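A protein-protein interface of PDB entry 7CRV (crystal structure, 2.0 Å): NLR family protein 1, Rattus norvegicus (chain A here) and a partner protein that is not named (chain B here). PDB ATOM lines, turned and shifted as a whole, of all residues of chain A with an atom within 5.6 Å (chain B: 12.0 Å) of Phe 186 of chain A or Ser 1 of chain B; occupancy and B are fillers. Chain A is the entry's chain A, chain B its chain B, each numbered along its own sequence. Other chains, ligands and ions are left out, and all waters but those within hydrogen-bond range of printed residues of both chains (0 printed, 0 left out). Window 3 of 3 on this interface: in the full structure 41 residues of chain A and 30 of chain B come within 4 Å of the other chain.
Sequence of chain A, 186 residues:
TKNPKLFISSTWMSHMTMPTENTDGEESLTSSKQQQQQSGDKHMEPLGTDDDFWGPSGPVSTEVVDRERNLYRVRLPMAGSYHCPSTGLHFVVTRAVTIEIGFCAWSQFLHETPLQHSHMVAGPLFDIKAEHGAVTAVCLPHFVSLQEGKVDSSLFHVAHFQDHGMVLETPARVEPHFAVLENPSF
The backbone carbonyl oxygen of Phe 126 of chain A sits at hydrogen-bond distance from the backbone NH of Met 3 of chain B (2.8 Å). The backbone NH (N) of Ser 1 of chain B sits at hydrogen-bond distance from a ring nitrogen (NE2) of His 160 of chain A (3.1 Å). OG of Ser 1 of chain B sits at hydrogen-bond distance from O of Phe 161 of chain A (2.7 Å). O of Pro 2 of chain B is in hydrogen-bond range of N of Phe 161 of chain A (3.0 Å).
The side-chain carboxylate (OD1) of Asp 127 of chain A lies within salt-bridge range of the side-chain amino group (NZ) of Lys 129 of chain A (3.9 Å).
Ser 1 of chain B touches Phe 126 of chain A. Pro 2 of chain B touches Phe 126 of chain A (CA to O, 3.3 Å). C of Ser 1 of chain B touches OD1 of Asp 127 of chain A, at 3.5 Å. Pro 2 of chain B touches Asp 127 of chain A. N of Ile 128 of chain A touches O of Ser 1 of chain B (3.8 Å). His 160 of chain A touches Pro 2 of chain B. His 160 of chain A touches Met 3 of chain B. Ser 1 of chain B touches Phe 186 of chain A (N to C, 3.1 Å). CD1 of Phe 186 of chain A touches CE of Met 3 of chain B (3.4 Å).
Printed residues of chain B within 4 Å of Phe 126 of chain A: Ser 1, Pro 2 and Met 3. Asp 127 of chain A touches just these residues of chain B: Ser 1 and Pro 2. Of chain B, only Ser 1 (3.8 Å) comes within 4 Å of Ile 128 of chain A. No residue of chain B comes within 4 Å of Lys 129 of chain A. No residue of chain B comes within 4 Å of Ala 130 of chain A. No residue of chain B comes within 4 Å of Val 135 of chain A. No residue of chain B comes within 4 Å of Val 138 of chain A. Of chain B, only Ser 1, Pro 2 and Met 3 come within 4 Å of His 160 of chain A. No residue of chain B comes within 4 Å of Gln 162 of chain A. No residue of chain B comes within 4 Å of Ser 185 of chain A. Phe 186 of chain A touches just these residues of chain B: Ser 1 (3.1 Å) and Met 3 (3.4 Å). Of the printed residues of chain A, Ser 1 of chain B touches Phe 126 (3.8 Å), Asp 127 (3.5 Å), Ile 128 (3.8 Å), His 160 (3.1 Å), Phe 161 (2.7 Å) and Phe 186 (3.1 Å). Of the printed residues of chain A, Pro 2 of chain B touches Phe 126 (3.3 Å), Asp 127 (3.8 Å), His 160 (3.5 Å) and Phe 161 (3.0 Å). Of the printed residues of chain A, Met 3 of chain B touches Phe 126, His 160 and Phe 186. The nearest residue of chain B that does not touch Phe 186 of chain A is Pro 2 of chain B (6.8 Å).
Of the 15 printed residues of chain A, 6 touch a printed residue of chain B. Printed residues of chain A that touch a printed residue of chain B: Phe 126, Asp 127, Ile 128, His 160, Phe 161 and Phe 186. Hydrophobic or aromatic side chains of chain A within 4 Å of the printed part of chain B: His 160, Phe 161 and Phe 186. Of the 5 printed residues of chain B, 3 touch a printed residue of chain A. Among the printed residues, no Asp or Glu carboxylate lies within 4 Å of a Lys or Arg side-chain nitrogen of the other chain.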
ATOM      1  N   PHE A  91     -22.132 -18.652  32.884  1.00  0.00           N
ATOM      2  CA  PHE A  91     -22.407 -17.612  33.866  1.00  0.00           C
ATOM      3  C   PHE A  91     -22.367 -18.236  35.251  1.00  0.00           C
ATOM      4  O   PHE A  91     -22.897 -19.338  35.449  1.00  0.00           O
ATOM      5  CB  PHE A  91     -23.765 -16.949  33.630  1.00  0.00           C
ATOM      6  CG  PHE A  91     -23.824 -16.129  32.359  1.00  0.00           C
ATOM      7  CD1 PHE A  91     -23.293 -14.842  32.321  1.00  0.00           C
ATOM      8  CD2 PHE A  91     -24.409 -16.647  31.214  1.00  0.00           C
ATOM      9  CE1 PHE A  91     -23.350 -14.085  31.159  1.00  0.00           C
ATOM     10  CE2 PHE A  91     -24.468 -15.904  30.045  1.00  0.00           C
ATOM     11  CZ  PHE A  91     -23.944 -14.623  30.019  1.00  0.00           C
ATOM     12  N   PHE A 126     -20.629 -10.786  22.063  1.00  0.00           N
ATOM     13  CA  PHE A 126     -21.962 -10.784  22.662  1.00  0.00           C
ATOM     14  C   PHE A 126     -22.259  -9.460  23.362  1.00  0.00           C
ATOM     15  O   PHE A 126     -21.427  -8.949  24.119  1.00  0.00           O
ATOM     16  CB  PHE A 126     -22.121 -11.886  23.723  1.00  0.00           C
ATOM     17  CG  PHE A 126     -21.815 -13.279  23.239  1.00  0.00           C
ATOM     18  CD1 PHE A 126     -22.770 -14.023  22.578  1.00  0.00           C
ATOM     19  CD2 PHE A 126     -20.584 -13.861  23.504  1.00  0.00           C
ATOM     20  CE1 PHE A 126     -22.492 -15.319  22.170  1.00  0.00           C
ATOM     21  CE2 PHE A 126     -20.301 -15.144  23.087  1.00  0.00           C
ATOM     22  CZ  PHE A 126     -21.251 -15.874  22.431  1.00  0.00           C
ATOM     23  N   ASP A 127     -23.475  -8.948  23.168  1.00  0.00           N
ATOM     24  CA  ASP A 127     -24.018  -7.867  23.989  1.00  0.00           C
ATOM     25  C   ASP A 127     -24.780  -8.501  25.148  1.00  0.00           C
ATOM     26  O   ASP A 127     -25.860  -9.068  24.950  1.00  0.00           O
ATOM     27  CB  ASP A 127     -24.942  -6.966  23.168  1.00  0.00           C
ATOM     28  CG  ASP A 127     -25.249  -5.623  23.858  1.00  0.00           C
ATOM     29  OD1 ASP A 127     -24.932  -5.446  25.058  1.00  0.00           O
ATOM     30  OD2 ASP A 127     -25.814  -4.734  23.184  1.00  0.00           O
ATOM     31  N   ILE A 128     -24.231  -8.404  26.356  1.00  0.00           N
ATOM     32  CA  ILE A 128     -24.820  -9.031  27.537  1.00  0.00           C
ATOM     33  C   ILE A 128     -25.311  -7.949  28.494  1.00  0.00           C
ATOM     34  O   ILE A 128     -24.627  -6.942  28.718  1.00  0.00           O
ATOM     35  CB  ILE A 128     -23.809  -9.987  28.208  1.00  0.00           C
ATOM     36  CG1 ILE A 128     -23.415 -11.097  27.214  1.00  0.00           C
ATOM     37  CG2 ILE A 128     -24.416 -10.613  29.460  1.00  0.00           C
ATOM     38  CD1 ILE A 128     -22.116 -11.812  27.500  1.00  0.00           C
ATOM     39  N   LYS A 129     -26.510  -8.144  29.040  1.00  0.00           N
ATOM     40  CA  LYS A 129     -27.093  -7.215  30.002  1.00  0.00           C
ATOM     41  C   LYS A 129     -27.624  -8.025  31.176  1.00  0.00           C
ATOM     42  O   LYS A 129     -28.403  -8.968  30.982  1.00  0.00           O
ATOM     43  CB  LYS A 129     -28.208  -6.378  29.367  1.00  0.00           C
ATOM     44  CG  LYS A 129     -27.760  -5.596  28.123  1.00  0.00           C
ATOM     45  CD  LYS A 129     -28.831  -4.601  27.669  1.00  0.00           C
ATOM     46  CE  LYS A 129     -28.635  -4.147  26.217  1.00  0.00           C
ATOM     47  NZ  LYS A 129     -27.740  -2.959  26.083  1.00  0.00           N
ATOM     48  N   ALA A 130     -27.172  -7.686  32.381  1.00  0.00           N
ATOM     49  CA  ALA A 130     -27.641  -8.321  33.605  1.00  0.00           C
ATOM     50  C   ALA A 130     -27.473  -7.331  34.745  1.00  0.00           C
ATOM     51  O   ALA A 130     -26.619  -6.446  34.684  1.00  0.00           O
ATOM     52  CB  ALA A 130     -26.889  -9.622  33.911  1.00  0.00           C
ATOM     53  N   VAL A 135     -23.851 -11.215  39.013  1.00  0.00           N
ATOM     54  CA  VAL A 135     -22.988 -12.080  38.214  1.00  0.00           C
ATOM     55  C   VAL A 135     -21.593 -12.106  38.826  1.00  0.00           C
ATOM     56  O   VAL A 135     -20.870 -11.102  38.781  1.00  0.00           O
ATOM     57  CB  VAL A 135     -22.944 -11.641  36.750  1.00  0.00           C
ATOM     58  CG1 VAL A 135     -21.934 -12.506  35.990  1.00  0.00           C
ATOM     59  CG2 VAL A 135     -24.340 -11.762  36.121  1.00  0.00           C
ATOM     60  N   VAL A 138     -18.445 -14.245  34.122  1.00  0.00           N
ATOM     61  CA  VAL A 138     -18.873 -14.720  32.811  1.00  0.00           C
ATOM     62  C   VAL A 138     -17.680 -15.403  32.165  1.00  0.00           C
ATOM     63  O   VAL A 138     -16.536 -14.978  32.351  1.00  0.00           O
ATOM     64  CB  VAL A 138     -19.425 -13.576  31.935  1.00  0.00           C
ATOM     65  CG1 VAL A 138     -18.393 -12.472  31.762  1.00  0.00           C
ATOM     66  CG2 VAL A 138     -19.872 -14.107  30.590  1.00  0.00           C
ATOM     67  N   HIS A 160     -14.292  -4.723  25.571  1.00  0.00           N
ATOM     68  CA  HIS A 160     -15.558  -4.248  26.101  1.00  0.00           C
ATOM     69  C   HIS A 160     -15.791  -2.901  25.440  1.00  0.00           C
ATOM     70  O   HIS A 160     -15.013  -1.967  25.667  1.00  0.00           O
ATOM     71  CB  HIS A 160     -15.488  -4.142  27.622  1.00  0.00           C
ATOM     72  CG  HIS A 160     -16.825  -4.069  28.284  1.00  0.00           C
ATOM     73  ND1 HIS A 160     -16.969  -3.925  29.647  1.00  0.00           N
ATOM     74  CD2 HIS A 160     -18.082  -4.098  27.774  1.00  0.00           C
ATOM     75  CE1 HIS A 160     -18.255  -3.881  29.949  1.00  0.00           C
ATOM     76  NE2 HIS A 160     -18.953  -3.989  28.832  1.00  0.00           N
ATOM     77  N   PHE A 161     -16.799  -2.816  24.565  1.00  0.00           N
ATOM     78  CA  PHE A 161     -17.009  -1.612  23.753  1.00  0.00           C
ATOM     79  C   PHE A 161     -18.081  -0.767  24.414  1.00  0.00           C
ATOM     80  O   PHE A 161     -19.275  -0.960  24.201  1.00  0.00           O
ATOM     81  CB  PHE A 161     -17.395  -1.954  22.316  1.00  0.00           C
ATOM     82  CG  PHE A 161     -16.372  -2.733  21.597  1.00  0.00           C
ATOM     83  CD1 PHE A 161     -15.299  -2.096  20.996  1.00  0.00           C
ATOM     84  CD2 PHE A 161     -16.457  -4.118  21.540  1.00  0.00           C
ATOM     85  CE1 PHE A 161     -14.329  -2.818  20.331  1.00  0.00           C
ATOM     86  CE2 PHE A 161     -15.494  -4.854  20.870  1.00  0.00           C
ATOM     87  CZ  PHE A 161     -14.425  -4.203  20.264  1.00  0.00           C
ATOM     88  N   GLN A 162     -17.641   0.180  25.212  1.00  0.00           N
ATOM     89  CA  GLN A 162     -18.536   1.139  25.843  1.00  0.00           C
ATOM     90  C   GLN A 162     -18.535   2.443  25.031  1.00  0.00           C
ATOM     91  O   GLN A 162     -17.617   2.701  24.223  1.00  0.00           O
ATOM     92  CB  GLN A 162     -18.100   1.368  27.287  1.00  0.00           C
ATOM     93  CG  GLN A 162     -17.732   0.017  27.984  1.00  0.00           C
ATOM     94  CD  GLN A 162     -17.748   0.001  29.524  1.00  0.00           C
ATOM     95  OE1 GLN A 162     -18.786  -0.248  30.152  1.00  0.00           O
ATOM     96  NE2 GLN A 162     -16.575   0.202  30.129  1.00  0.00           N
ATOM     97  N   ASP A 163     -19.618   3.202  25.185  1.00  0.00           N
ATOM     98  CA  ASP A 163     -19.736   4.598  24.830  1.00  0.00           C
ATOM     99  C   ASP A 163     -18.459   5.368  24.553  1.00  0.00           C
ATOM    100  O   ASP A 163     -18.377   5.963  23.475  1.00  0.00           O
ATOM    101  CB  ASP A 163     -20.609   5.204  25.929  1.00  0.00           C
ATOM    102  CG  ASP A 163     -22.057   5.100  25.605  1.00  0.00           C
ATOM    103  OD1 ASP A 163     -22.390   5.778  24.603  1.00  0.00           O
ATOM    104  OD2 ASP A 163     -22.746   4.108  26.121  1.00  0.00           O
ATOM    105  N   PRO A 184     -18.237  -8.891  36.163  1.00  0.00           N
ATOM    106  CA  PRO A 184     -18.422  -8.010  35.003  1.00  0.00           C
ATOM    107  C   PRO A 184     -19.488  -6.962  35.261  1.00  0.00           C
ATOM    108  O   PRO A 184     -20.533  -7.238  35.862  1.00  0.00           O
ATOM    109  CB  PRO A 184     -18.845  -8.974  33.893  1.00  0.00           C
ATOM    110  CG  PRO A 184     -19.470 -10.101  34.593  1.00  0.00           C
ATOM    111  CD  PRO A 184     -18.684 -10.262  35.872  1.00  0.00           C
ATOM    112  N   SER A 185     -19.192  -5.729  34.832  1.00  0.00           N
ATOM    113  CA  SER A 185     -20.186  -4.665  34.734  1.00  0.00           C
ATOM    114  C   SER A 185     -20.590  -4.571  33.259  1.00  0.00           C
ATOM    115  O   SER A 185     -19.884  -3.986  32.426  1.00  0.00           O
ATOM    116  CB  SER A 185     -19.668  -3.342  35.272  1.00  0.00           C
ATOM    117  OG  SER A 185     -19.523  -3.383  36.698  1.00  0.00           O
ATOM    118  N   PHE A 186     -21.728  -5.164  32.927  1.00  0.00           N
ATOM    119  CA  PHE A 186     -22.102  -5.249  31.538  1.00  0.00           C
ATOM    120  C   PHE A 186     -22.525  -3.879  31.018  1.00  0.00           C
ATOM    121  O   PHE A 186     -23.115  -3.080  31.750  1.00  0.00           O
ATOM    122  CB  PHE A 186     -23.216  -6.268  31.351  1.00  0.00           C
ATOM    123  CG  PHE A 186     -22.859  -7.641  31.808  1.00  0.00           C
ATOM    124  CD1 PHE A 186     -22.019  -8.452  31.049  1.00  0.00           C
ATOM    125  CD2 PHE A 186     -23.352  -8.118  33.007  1.00  0.00           C
ATOM    126  CE1 PHE A 186     -21.686  -9.729  31.473  1.00  0.00           C
ATOM    127  CE2 PHE A 186     -23.024  -9.386  33.443  1.00  0.00           C
ATOM    128  CZ  PHE A 186     -22.198 -10.196  32.671  1.00  0.00           C
ATOM    129  N   SER B   1     -21.956  -4.076  27.994  1.00  0.00           N
ATOM    130  CA  SER B   1     -22.123  -3.582  26.616  1.00  0.00           C
ATOM    131  C   SER B   1     -21.535  -4.757  25.743  1.00  0.00           C
ATOM    132  O   SER B   1     -21.420  -5.854  26.290  1.00  0.00           O
ATOM    133  CB  SER B   1     -21.436  -2.202  26.520  1.00  0.00           C
ATOM    134  OG  SER B   1     -21.678  -1.510  25.311  1.00  0.00           O
ATOM    135  N   PRO B   2     -21.235  -4.617  24.430  1.00  0.00           N
ATOM    136  CA  PRO B   2     -20.689  -5.781  23.703  1.00  0.00           C
ATOM    137  C   PRO B   2     -19.306  -6.160  24.209  1.00  0.00           C
ATOM    138  O   PRO B   2     -18.478  -5.290  24.487  1.00  0.00           O
ATOM    139  CB  PRO B   2     -20.621  -5.304  22.245  1.00  0.00           C
ATOM    140  CG  PRO B   2     -21.581  -4.201  22.153  1.00  0.00           C
ATOM    141  CD  PRO B   2     -21.549  -3.532  23.482  1.00  0.00           C
ATOM    142  N   MET B   3     -19.046  -7.471  24.290  1.00  0.00           N
ATOM    143  CA  MET B   3     -17.766  -7.974  24.792  1.00  0.00           C
ATOM    144  C   MET B   3     -17.471  -9.360  24.214  1.00  0.00           C
ATOM    145  O   MET B   3     -18.380 -10.121  23.860  1.00  0.00           O
ATOM    146  CB  MET B   3     -17.740  -8.011  26.348  1.00  0.00           C
ATOM    147  CG  MET B   3     -18.798  -8.919  26.965  1.00  0.00           C
ATOM    148  SD  MET B   3     -18.696  -9.069  28.782  1.00  0.00           S
ATOM    149  CE  MET B   3     -19.282  -7.446  29.279  1.00  0.00           C
ATOM    150  N   GLY B   4     -16.186  -9.669  24.114  1.00  0.00           N
ATOM    151  CA  GLY B   4     -15.721 -10.923  23.543  1.00  0.00           C
ATOM    152  C   GLY B   4     -14.213 -10.920  23.621  1.00  0.00           C
ATOM    153  O   GLY B   4     -13.607  -9.937  24.046  1.00  0.00           O
ATOM    154  N   VAL B   5     -13.600 -12.006  23.144  1.00  0.00           N
ATOM    155  CA  VAL B   5     -12.175 -12.273  23.362  1.00  0.00           C
ATOM    156  C   VAL B   5     -11.340 -11.874  22.138  1.00  0.00           C
ATOM    157  O   VAL B   5     -11.664 -12.237  21.000  1.00  0.00           O
ATOM    158  CB  VAL B   5     -11.953 -13.747  23.729  1.00  0.00           C
ATOM    159  CG1 VAL B   5     -10.447 -14.037  23.942  1.00  0.00           C
ATOM    160  CG2 VAL B   5     -12.771 -14.090  25.007  1.00  0.00           C
